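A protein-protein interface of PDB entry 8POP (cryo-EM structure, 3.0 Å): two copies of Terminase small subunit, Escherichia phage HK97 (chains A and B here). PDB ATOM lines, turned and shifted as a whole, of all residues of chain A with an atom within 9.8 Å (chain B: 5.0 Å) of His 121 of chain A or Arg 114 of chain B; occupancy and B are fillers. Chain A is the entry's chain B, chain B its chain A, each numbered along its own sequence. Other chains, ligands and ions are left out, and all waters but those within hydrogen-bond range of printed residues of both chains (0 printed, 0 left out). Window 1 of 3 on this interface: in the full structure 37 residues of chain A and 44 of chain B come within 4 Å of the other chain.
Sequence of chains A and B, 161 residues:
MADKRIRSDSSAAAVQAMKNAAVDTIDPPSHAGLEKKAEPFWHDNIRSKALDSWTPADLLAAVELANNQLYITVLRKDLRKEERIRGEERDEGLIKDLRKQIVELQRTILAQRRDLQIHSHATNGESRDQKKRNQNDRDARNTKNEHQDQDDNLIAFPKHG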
ATOM      1  N   SER A  48      24.199 -23.431  17.150  1.00  0.00           N
ATOM      2  CA  SER A  48      23.731 -22.108  17.534  1.00  0.00           C
ATOM      3  C   SER A  48      23.401 -21.220  16.340  1.00  0.00           C
ATOM      4  O   SER A  48      23.190 -20.024  16.526  1.00  0.00           O
ATOM      5  CB  SER A  48      24.713 -21.440  18.433  1.00  0.00           C
ATOM      6  OG  SER A  48      24.726 -22.083  19.700  1.00  0.00           O
ATOM      7  N   ARG A 107      38.714 -12.793  26.327  1.00  0.00           N
ATOM      8  CA  ARG A 107      38.430 -11.709  25.405  1.00  0.00           C
ATOM      9  C   ARG A 107      38.558 -12.184  23.951  1.00  0.00           C
ATOM     10  O   ARG A 107      37.797 -11.763  23.097  1.00  0.00           O
ATOM     11  CB  ARG A 107      39.362 -10.530  25.667  1.00  0.00           C
ATOM     12  CG  ARG A 107      39.048  -9.761  26.933  1.00  0.00           C
ATOM     13  CD  ARG A 107      38.082  -8.668  26.581  1.00  0.00           C
ATOM     14  NE  ARG A 107      38.017  -7.583  27.553  1.00  0.00           N
ATOM     15  CZ  ARG A 107      37.430  -6.423  27.322  1.00  0.00           C
ATOM     16  NH1 ARG A 107      36.751  -6.212  26.207  1.00  0.00           N
ATOM     17  NH2 ARG A 107      37.501  -5.464  28.232  1.00  0.00           N
ATOM     18  N   LEU A 110      35.365 -13.891  22.825  1.00  0.00           N
ATOM     19  CA  LEU A 110      34.308 -12.970  22.409  1.00  0.00           C
ATOM     20  C   LEU A 110      34.512 -12.525  20.963  1.00  0.00           C
ATOM     21  O   LEU A 110      33.557 -12.419  20.234  1.00  0.00           O
ATOM     22  CB  LEU A 110      34.234 -11.760  23.338  1.00  0.00           C
ATOM     23  CG  LEU A 110      33.785 -12.059  24.766  1.00  0.00           C
ATOM     24  CD1 LEU A 110      33.302 -10.829  25.500  1.00  0.00           C
ATOM     25  CD2 LEU A 110      32.666 -13.039  24.792  1.00  0.00           C
ATOM     26  N   ARG A 113      33.543 -15.421  18.588  1.00  0.00           N
ATOM     27  CA  ARG A 113      32.097 -15.594  18.482  1.00  0.00           C
ATOM     28  C   ARG A 113      31.533 -14.575  17.503  1.00  0.00           C
ATOM     29  O   ARG A 113      30.743 -14.931  16.655  1.00  0.00           O
ATOM     30  CB  ARG A 113      31.424 -15.483  19.848  1.00  0.00           C
ATOM     31  CG  ARG A 113      31.426 -16.790  20.631  1.00  0.00           C
ATOM     32  CD  ARG A 113      31.163 -16.597  22.116  1.00  0.00           C
ATOM     33  NE  ARG A 113      30.016 -15.771  22.486  1.00  0.00           N
ATOM     34  CZ  ARG A 113      28.738 -16.113  22.294  1.00  0.00           C
ATOM     35  NH1 ARG A 113      27.788 -15.669  23.100  1.00  0.00           N
ATOM     36  NH2 ARG A 113      28.415 -16.917  21.297  1.00  0.00           N
ATOM     37  N   ARG A 114      31.945 -13.309  17.633  1.00  0.00           N
ATOM     38  CA  ARG A 114      31.467 -12.219  16.790  1.00  0.00           C
ATOM     39  C   ARG A 114      31.760 -12.504  15.330  1.00  0.00           C
ATOM     40  O   ARG A 114      30.931 -12.238  14.474  1.00  0.00           O
ATOM     41  CB  ARG A 114      32.123 -10.903  17.160  1.00  0.00           C
ATOM     42  CG  ARG A 114      31.394 -10.134  18.219  1.00  0.00           C
ATOM     43  CD  ARG A 114      32.052  -8.786  18.534  1.00  0.00           C
ATOM     44  NE  ARG A 114      33.499  -8.757  18.443  1.00  0.00           N
ATOM     45  CZ  ARG A 114      34.350  -8.647  19.459  1.00  0.00           C
ATOM     46  NH1 ARG A 114      35.655  -8.623  19.217  1.00  0.00           N
ATOM     47  NH2 ARG A 114      33.930  -8.548  20.711  1.00  0.00           N
ATOM     48  N   GLN A 117      29.333 -14.809  13.809  1.00  0.00           N
ATOM     49  CA  GLN A 117      27.957 -14.379  13.976  1.00  0.00           C
ATOM     50  C   GLN A 117      27.187 -15.401  14.792  1.00  0.00           C
ATOM     51  O   GLN A 117      26.077 -15.740  14.403  1.00  0.00           O
ATOM     52  CB  GLN A 117      27.295 -14.187  12.600  1.00  0.00           C
ATOM     53  CG  GLN A 117      27.965 -13.154  11.699  1.00  0.00           C
ATOM     54  CD  GLN A 117      27.636 -11.751  12.115  1.00  0.00           C
ATOM     55  OE1 GLN A 117      28.489 -10.913  12.424  1.00  0.00           O
ATOM     56  NE2 GLN A 117      26.349 -11.480  12.078  1.00  0.00           N
ATOM     57  N   ILE A 118      27.738 -15.900  15.890  1.00  0.00           N
ATOM     58  CA  ILE A 118      26.926 -16.706  16.802  1.00  0.00           C
ATOM     59  C   ILE A 118      26.831 -16.019  18.158  1.00  0.00           C
ATOM     60  O   ILE A 118      26.428 -16.657  19.133  1.00  0.00           O
ATOM     61  CB  ILE A 118      27.447 -18.156  16.956  1.00  0.00           C
ATOM     62  CG1 ILE A 118      28.825 -18.210  17.626  1.00  0.00           C
ATOM     63  CG2 ILE A 118      27.454 -18.844  15.617  1.00  0.00           C
ATOM     64  CD1 ILE A 118      29.464 -19.577  17.689  1.00  0.00           C
ATOM     65  N   HIS A 119      27.196 -14.731  18.216  1.00  0.00           N
ATOM     66  CA  HIS A 119      26.964 -13.997  19.450  1.00  0.00           C
ATOM     67  C   HIS A 119      25.502 -13.542  19.472  1.00  0.00           C
ATOM     68  O   HIS A 119      24.865 -13.460  18.433  1.00  0.00           O
ATOM     69  CB  HIS A 119      27.944 -12.824  19.597  1.00  0.00           C
ATOM     70  CG  HIS A 119      27.813 -11.799  18.522  1.00  0.00           C
ATOM     71  ND1 HIS A 119      27.839 -12.119  17.156  1.00  0.00           N
ATOM     72  CD2 HIS A 119      27.650 -10.478  18.643  1.00  0.00           C
ATOM     73  CE1 HIS A 119      27.711 -10.981  16.483  1.00  0.00           C
ATOM     74  NE2 HIS A 119      27.584  -9.987  17.351  1.00  0.00           N
ATOM     75  N   SER A 120      25.027 -13.187  20.657  1.00  0.00           N
ATOM     76  CA  SER A 120      23.629 -12.930  20.896  1.00  0.00           C
ATOM     77  C   SER A 120      23.060 -11.872  19.954  1.00  0.00           C
ATOM     78  O   SER A 120      21.945 -12.020  19.464  1.00  0.00           O
ATOM     79  CB  SER A 120      23.421 -12.543  22.350  1.00  0.00           C
ATOM     80  OG  SER A 120      22.042 -12.466  22.706  1.00  0.00           O
ATOM     81  N   HIS A 121      23.801 -10.807  19.701  1.00  0.00           N
ATOM     82  CA  HIS A 121      23.294  -9.705  18.893  1.00  0.00           C
ATOM     83  C   HIS A 121      22.883 -10.209  17.510  1.00  0.00           C
ATOM     84  O   HIS A 121      21.906  -9.738  16.935  1.00  0.00           O
ATOM     85  CB  HIS A 121      24.299  -8.555  18.737  1.00  0.00           C
ATOM     86  CG  HIS A 121      24.675  -7.910  20.026  1.00  0.00           C
ATOM     87  ND1 HIS A 121      24.348  -6.623  20.396  1.00  0.00           N
ATOM     88  CD2 HIS A 121      25.277  -8.439  21.089  1.00  0.00           C
ATOM     89  CE1 HIS A 121      24.748  -6.411  21.645  1.00  0.00           C
ATOM     90  NE2 HIS A 121      25.320  -7.504  22.084  1.00  0.00           N
ATOM     91  N   ALA A 122      23.641 -11.156  16.969  1.00  0.00           N
ATOM     92  CA  ALA A 122      23.415 -11.637  15.621  1.00  0.00           C
ATOM     93  C   ALA A 122      22.343 -12.708  15.585  1.00  0.00           C
ATOM     94  O   ALA A 122      21.771 -12.948  14.521  1.00  0.00           O
ATOM     95  CB  ALA A 122      24.690 -12.168  15.074  1.00  0.00           C
ATOM     96  N   THR A 123      22.060 -13.344  16.729  1.00  0.00           N
ATOM     97  CA  THR A 123      21.098 -14.440  16.766  1.00  0.00           C
ATOM     98  C   THR A 123      19.778 -13.996  17.399  1.00  0.00           C
ATOM     99  O   THR A 123      18.843 -14.779  17.468  1.00  0.00           O
ATOM    100  CB  THR A 123      21.664 -15.634  17.539  1.00  0.00           C
ATOM    101  OG1 THR A 123      21.843 -15.264  18.909  1.00  0.00           O
ATOM    102  CG2 THR A 123      22.991 -16.135  17.008  1.00  0.00           C
ATOM    103  N   ASN A 124      19.707 -12.709  17.772  1.00  0.00           N
ATOM    104  CA  ASN A 124      18.497 -12.093  18.276  1.00  0.00           C
ATOM    105  C   ASN A 124      18.287 -10.664  17.765  1.00  0.00           C
ATOM    106  O   ASN A 124      17.182 -10.153  17.874  1.00  0.00           O
ATOM    107  CB  ASN A 124      18.510 -12.041  19.794  1.00  0.00           C
ATOM    108  CG  ASN A 124      18.769 -13.402  20.376  1.00  0.00           C
ATOM    109  OD1 ASN A 124      19.706 -13.611  21.144  1.00  0.00           O
ATOM    110  ND2 ASN A 124      17.919 -14.342  20.025  1.00  0.00           N
ATOM    111  N   GLY A 125      19.328  -9.964  17.305  1.00  0.00           N
ATOM    112  CA  GLY A 125      19.171  -8.641  16.697  1.00  0.00           C
ATOM    113  C   GLY A 125      19.618  -7.442  17.553  1.00  0.00           C
ATOM    114  O   GLY A 125      20.220  -7.586  18.609  1.00  0.00           O
ATOM    115  N   GLU A 126      19.284  -6.231  17.112  1.00  0.00           N
ATOM    116  CA  GLU A 126      19.620  -5.043  17.877  1.00  0.00           C
ATOM    117  C   GLU A 126      19.019  -5.031  19.273  1.00  0.00           C
ATOM    118  O   GLU A 126      17.826  -5.216  19.481  1.00  0.00           O
ATOM    119  CB  GLU A 126      19.106  -3.756  17.235  1.00  0.00           C
ATOM    120  CG  GLU A 126      19.840  -3.406  15.951  1.00  0.00           C
ATOM    121  CD  GLU A 126      19.219  -2.300  15.117  1.00  0.00           C
ATOM    122  OE1 GLU A 126      18.184  -1.719  15.542  1.00  0.00           O
ATOM    123  OE2 GLU A 126      19.760  -2.040  14.026  1.00  0.00           O
ATOM    124  N   SER A 127      19.882  -4.671  20.213  1.00  0.00           N
ATOM    125  CA  SER A 127      19.506  -4.502  21.598  1.00  0.00           C
ATOM    126  C   SER A 127      18.111  -3.885  21.710  1.00  0.00           C
ATOM    127  O   SER A 127      17.275  -4.423  22.411  1.00  0.00           O
ATOM    128  CB  SER A 127      20.560  -3.666  22.291  1.00  0.00           C
ATOM    129  OG  SER A 127      21.838  -4.286  22.267  1.00  0.00           O
ATOM    130  N   ARG A 128      17.850  -2.757  21.039  1.00  0.00           N
ATOM    131  CA  ARG A 128      16.613  -2.025  21.278  1.00  0.00           C
ATOM    132  C   ARG A 128      15.420  -2.875  20.842  1.00  0.00           C
ATOM    133  O   ARG A 128      14.294  -2.635  21.261  1.00  0.00           O
ATOM    134  CB  ARG A 128      16.577  -0.657  20.574  1.00  0.00           C
ATOM    135  CG  ARG A 128      16.476  -0.717  19.056  1.00  0.00           C
ATOM    136  CD  ARG A 128      16.547   0.604  18.303  1.00  0.00           C
ATOM    137  NE  ARG A 128      16.824   0.398  16.879  1.00  0.00           N
ATOM    138  CZ  ARG A 128      17.130   1.349  15.988  1.00  0.00           C
ATOM    139  NH1 ARG A 128      17.110   2.631  16.313  1.00  0.00           N
ATOM    140  NH2 ARG A 128      17.478   1.002  14.757  1.00  0.00           N
ATOM    141  N   ASP A 129      15.666  -3.883  20.014  1.00  0.00           N
ATOM    142  CA  ASP A 129      14.584  -4.716  19.551  1.00  0.00           C
ATOM    143  C   ASP A 129      14.440  -5.951  20.446  1.00  0.00           C
ATOM    144  O   ASP A 129      13.865  -6.971  20.068  1.00  0.00           O
ATOM    145  CB  ASP A 129      14.836  -5.023  18.078  1.00  0.00           C
ATOM    146  CG  ASP A 129      14.725  -3.795  17.183  1.00  0.00           C
ATOM    147  OD1 ASP A 129      14.252  -2.732  17.673  1.00  0.00           O
ATOM    148  OD2 ASP A 129      15.114  -3.906  15.990  1.00  0.00           O
ATOM    149  N   GLN A 130      14.989  -5.885  21.646  1.00  0.00           N
ATOM    150  CA  GLN A 130      14.813  -6.973  22.573  1.00  0.00           C
ATOM    151  C   GLN A 130      14.044  -6.444  23.761  1.00  0.00           C
ATOM    152  O   GLN A 130      13.780  -7.190  24.697  1.00  0.00           O
ATOM    153  CB  GLN A 130      16.155  -7.469  23.070  1.00  0.00           C
ATOM    154  CG  GLN A 130      17.156  -7.628  21.942  1.00  0.00           C
ATOM    155  CD  GLN A 130      16.797  -8.793  21.065  1.00  0.00           C
ATOM    156  OE1 GLN A 130      16.564  -9.899  21.548  1.00  0.00           O
ATOM    157  NE2 GLN A 130      16.799  -8.556  19.766  1.00  0.00           N
ATOM    158  N   ARG A 133      10.040  -8.092  24.124  1.00  0.00           N
ATOM    159  CA  ARG A 133      10.170  -9.523  24.326  1.00  0.00           C
ATOM    160  C   ARG A 133      10.443  -9.796  25.793  1.00  0.00           C
ATOM    161  O   ARG A 133       9.749 -10.564  26.429  1.00  0.00           O
ATOM    162  CB  ARG A 133      11.319 -10.006  23.450  1.00  0.00           C
ATOM    163  CG  ARG A 133      11.621 -11.491  23.490  1.00  0.00           C
ATOM    164  CD  ARG A 133      12.560 -11.732  22.321  1.00  0.00           C
ATOM    165  NE  ARG A 133      12.888 -13.131  22.149  1.00  0.00           N
ATOM    166  CZ  ARG A 133      13.669 -13.604  21.187  1.00  0.00           C
ATOM    167  NH1 ARG A 133      14.175 -12.781  20.283  1.00  0.00           N
ATOM    168  NH2 ARG A 133      13.922 -14.902  21.129  1.00  0.00           N
ATOM    169  N   LEU B 110      31.863  -6.428  32.287  1.00  0.00           N
ATOM    170  CA  LEU B 110      30.992  -5.541  31.543  1.00  0.00           C
ATOM    171  C   LEU B 110      30.914  -5.963  30.076  1.00  0.00           C
ATOM    172  O   LEU B 110      29.828  -5.915  29.488  1.00  0.00           O
ATOM    173  CB  LEU B 110      31.488  -4.088  31.630  1.00  0.00           C
ATOM    174  CG  LEU B 110      31.384  -3.422  32.987  1.00  0.00           C
ATOM    175  CD1 LEU B 110      31.452  -1.906  32.844  1.00  0.00           C
ATOM    176  CD2 LEU B 110      30.074  -3.815  33.670  1.00  0.00           C
ATOM    177  N   ALA B 111      32.042  -6.348  29.473  1.00  0.00           N
ATOM    178  CA  ALA B 111      32.033  -6.763  28.088  1.00  0.00           C
ATOM    179  C   ALA B 111      31.215  -8.032  27.911  1.00  0.00           C
ATOM    180  O   ALA B 111      30.492  -8.137  26.919  1.00  0.00           O
ATOM    181  CB  ALA B 111      33.437  -7.033  27.602  1.00  0.00           C
ATOM    182  N   GLN B 112      31.382  -9.001  28.836  1.00  0.00           N
ATOM    183  CA  GLN B 112      30.675 -10.256  28.737  1.00  0.00           C
ATOM    184  C   GLN B 112      29.170  -9.994  28.778  1.00  0.00           C
ATOM    185  O   GLN B 112      28.438 -10.555  27.967  1.00  0.00           O
ATOM    186  CB  GLN B 112      31.115 -11.204  29.854  1.00  0.00           C
ATOM    187  CG  GLN B 112      32.515 -11.765  29.637  1.00  0.00           C
ATOM    188  CD  GLN B 112      33.047 -12.525  30.841  1.00  0.00           C
ATOM    189  OE1 GLN B 112      33.094 -12.015  31.960  1.00  0.00           O
ATOM    190  NE2 GLN B 112      33.470 -13.765  30.647  1.00  0.00           N
ATOM    191  N   ARG B 113      28.713  -9.143  29.718  1.00  0.00           N
ATOM    192  CA  ARG B 113      27.293  -8.885  29.840  1.00  0.00           C
ATOM    193  C   ARG B 113      26.749  -8.336  28.517  1.00  0.00           C
ATOM    194  O   ARG B 113      25.719  -8.781  28.048  1.00  0.00           O
ATOM    195  CB  ARG B 113      26.998  -7.892  30.955  1.00  0.00           C
ATOM    196  CG  ARG B 113      26.909  -8.449  32.358  1.00  0.00           C
ATOM    197  CD  ARG B 113      27.132  -7.361  33.422  1.00  0.00           C
ATOM    198  NE  ARG B 113      26.308  -6.172  33.276  1.00  0.00           N
ATOM    199  CZ  ARG B 113      25.008  -6.102  33.528  1.00  0.00           C
ATOM    200  NH1 ARG B 113      24.384  -7.174  33.986  1.00  0.00           N
ATOM    201  NH2 ARG B 113      24.343  -4.951  33.403  1.00  0.00           N
ATOM    202  N   ARG B 114      27.437  -7.371  27.915  1.00  0.00           N
ATOM    203  CA  ARG B 114      26.990  -6.732  26.681  1.00  0.00           C
ATOM    204  C   ARG B 114      26.865  -7.759  25.563  1.00  0.00           C
ATOM    205  O   ARG B 114      25.936  -7.711  24.774  1.00  0.00           O
ATOM    206  CB  ARG B 114      28.002  -5.666  26.236  1.00  0.00           C
ATOM    207  CG  ARG B 114      27.389  -4.630  25.308  1.00  0.00           C
ATOM    208  CD  ARG B 114      28.222  -3.379  25.179  1.00  0.00           C
ATOM    209  NE  ARG B 114      29.568  -3.763  24.780  1.00  0.00           N
ATOM    210  CZ  ARG B 114      30.690  -3.414  25.399  1.00  0.00           C
ATOM    211  NH1 ARG B 114      31.846  -3.915  24.967  1.00  0.00           N
ATOM    212  NH2 ARG B 114      30.642  -2.583  26.434  1.00  0.00           N
ATOM    213  N   ASP B 115      27.801  -8.704  25.512  1.00  0.00           N
ATOM    214  CA  ASP B 115      27.837  -9.711  24.468  1.00  0.00           C
ATOM    215  C   ASP B 115      26.626 -10.634  24.555  1.00  0.00           C
ATOM    216  O   ASP B 115      26.209 -11.170  23.538  1.00  0.00           O
ATOM    217  CB  ASP B 115      29.096 -10.562  24.589  1.00  0.00           C
ATOM    218  CG  ASP B 115      29.133 -11.780  23.684  1.00  0.00           C
ATOM    219  OD1 ASP B 115      29.447 -11.617  22.486  1.00  0.00           O
ATOM    220  OD2 ASP B 115      28.853 -12.890  24.192  1.00  0.00           O
ATOM    221  N   LEU B 116      26.102 -10.865  25.765  1.00  0.00           N
ATOM    222  CA  LEU B 116      24.958 -11.753  25.936  1.00  0.00           C
ATOM    223  C   LEU B 116      23.643 -10.959  25.910  1.00  0.00           C
ATOM    224  O   LEU B 116      22.588 -11.520  26.050  1.00  0.00           O
ATOM    225  CB  LEU B 116      25.094 -12.493  27.265  1.00  0.00           C
ATOM    226  CG  LEU B 116      26.184 -13.536  27.321  1.00  0.00           C
ATOM    227  CD1 LEU B 116      26.330 -14.052  28.765  1.00  0.00           C
ATOM    228  CD2 LEU B 116      25.879 -14.644  26.391  1.00  0.00           C
ATOM    229  N   GLN B 117      23.710  -9.666  25.749  1.00  0.00           N
ATOM    230  CA  GLN B 117      22.525  -8.827  25.765  1.00  0.00           C
ATOM    231  C   GLN B 117      21.784  -8.984  27.077  1.00  0.00           C
ATOM    232  O   GLN B 117      20.568  -9.090  27.057  1.00  0.00           O
ATOM    233  CB  GLN B 117      21.590  -9.130  24.584  1.00  0.00           C
ATOM    234  CG  GLN B 117      22.260  -8.901  23.227  1.00  0.00           C
ATOM    235  CD  GLN B 117      21.301  -8.656  22.099  1.00  0.00           C
ATOM    236  OE1 GLN B 117      20.576  -9.571  21.729  1.00  0.00           O
ATOM    237  NE2 GLN B 117      21.303  -7.445  21.554  1.00  0.00           N
ATOM    238  N   HIS B 119      22.802  -6.600  29.392  1.00  0.00           N
ATOM    239  CA  HIS B 119      23.071  -5.268  29.921  1.00  0.00           C
ATOM    240  C   HIS B 119      21.795  -4.445  29.885  1.00  0.00           C
ATOM    241  O   HIS B 119      20.862  -4.766  29.140  1.00  0.00           O
ATOM    242  CB  HIS B 119      24.177  -4.575  29.137  1.00  0.00           C
ATOM    243  CG  HIS B 119      23.872  -4.350  27.694  1.00  0.00           C
ATOM    244  ND1 HIS B 119      23.453  -5.358  26.854  1.00  0.00           N
ATOM    245  CD2 HIS B 119      23.944  -3.227  26.958  1.00  0.00           C
ATOM    246  CE1 HIS B 119      23.266  -4.851  25.643  1.00  0.00           C
ATOM    247  NE2 HIS B 119      23.575  -3.548  25.680  1.00  0.00           N
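O of Arg 114 of chain B sits at hydrogen-bond distance from NE2 of His 121 of chain A, 2.8 Å away.
OD2 of Asp 115 of chain B is in salt-bridge range of NH1 of Arg 113 of chain A (3.2 Å).
OG of Ser 120 of chain A lies within hydrogen-bond range of OE1 of Gln 117 of chain B (3.4 Å).
The side-chain amide nitrogen (NE2) of Gln 117 of chain B lies within hydrogen-bond range of a ring nitrogen (ND1) of His 121 of chain A, at 3.4 Å.
NE2 of Gln 117 of chain B sits at hydrogen-bond distance from O of Gly 125 of chain A, at 3.1 Å.
The side-chain amide nitrogen (NE2) of Gln 117 of chain B sits at hydrogen-bond distance from the side-chain hydroxyl (OG) of Ser 127 of chain A (3.3 Å).
The guanidinium group (NH2) of Arg 113 of chain A sits at hydrogen-bond distance from the backbone carbonyl oxygen (O) of Ile 118 of chain A, at 2.9 Å.
The backbone carbonyl oxygen (O) of Ser 120 of chain A sits at hydrogen-bond distance from the side-chain hydroxyl (OG1) of Thr 123 of chain A.
The side-chain hydroxyl (OG) of Ser 120 of chain A sits at hydrogen-bond distance from the side-chain amide oxygen (OD1) of Asn 124 of chain A.
O of Asn 124 of chain A is in hydrogen-bond range of NE2 of Gln 130 of chain A (2.5 Å).
Of the 9 printed residues of chain B, 6 touch a printed residue of chain A.
Hydrophobic or aromatic side chains of chain B within 4 Å of the printed part of chain A: Ala 111, Leu 116 and His 119.
Printed residues of chain A that touch a printed residue of chain B: Arg 107, Leu 110, Arg 113, His 119, Ser 120, His 121, Asn 124, Gly 125, Ser 127 and Gln 130.
Among the printed residues, Asp or Glu carboxylates within 4 Å of a Lys or Arg side-chain nitrogen of the other chain: Arg 113 of chain A with Asp 115 of chain B (3.2 Å).
Among the printed residues, merely in contact across the chains: Arg 107 of chain A with Ala 111 of chain B (3.7 Å), Leu 110 of chain A with Asp 115 of chain B (3.9 Å), Arg 113 of chain A with Leu 116 of chain B (3.9 Å), His 119 of chain A with Asp 115 of chain B (3.5 Å), Ser 120 of chain A with Asp 115 of chain B (3.3 Å), Ser 120 of chain A with Leu 116 of chain B (3.5 Å), His 121 of chain A with Asp 115 of chain B (3.8 Å), Asn 124 of chain A with Gln 117 of chain B (3.8 Å), Ser 127 of chain A with His 119 of chain B (3.7 Å) and Gln 130 of chain A with Gln 117 of chain B (3.9 Å).
Of the printed residues of chain B, His 121 of chain A touches Arg 114 (2.8 Å), Asp 115 (3.8 Å) and Gln 117 (3.4 Å).
Of chain A, only His 121 (2.8 Å) comes within 4 Å of Arg 114 of chain B.
Of chain A, only Arg 107 comes within 4 Å of Ala 111 of chain B.
Of the printed residues of chain B, Leu 110 of chain A touches Asp 115.
Of the printed residues of chain B, Gln 130 of chain A touches Gln 117.
Printed residues of chain B within 4 Å of Arg 113 of chain A: Asp 115 and Leu 116.
Of the printed residues of chain B, Arg 107 of chain A touches Ala 111.
5 positions are printed for both chains.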
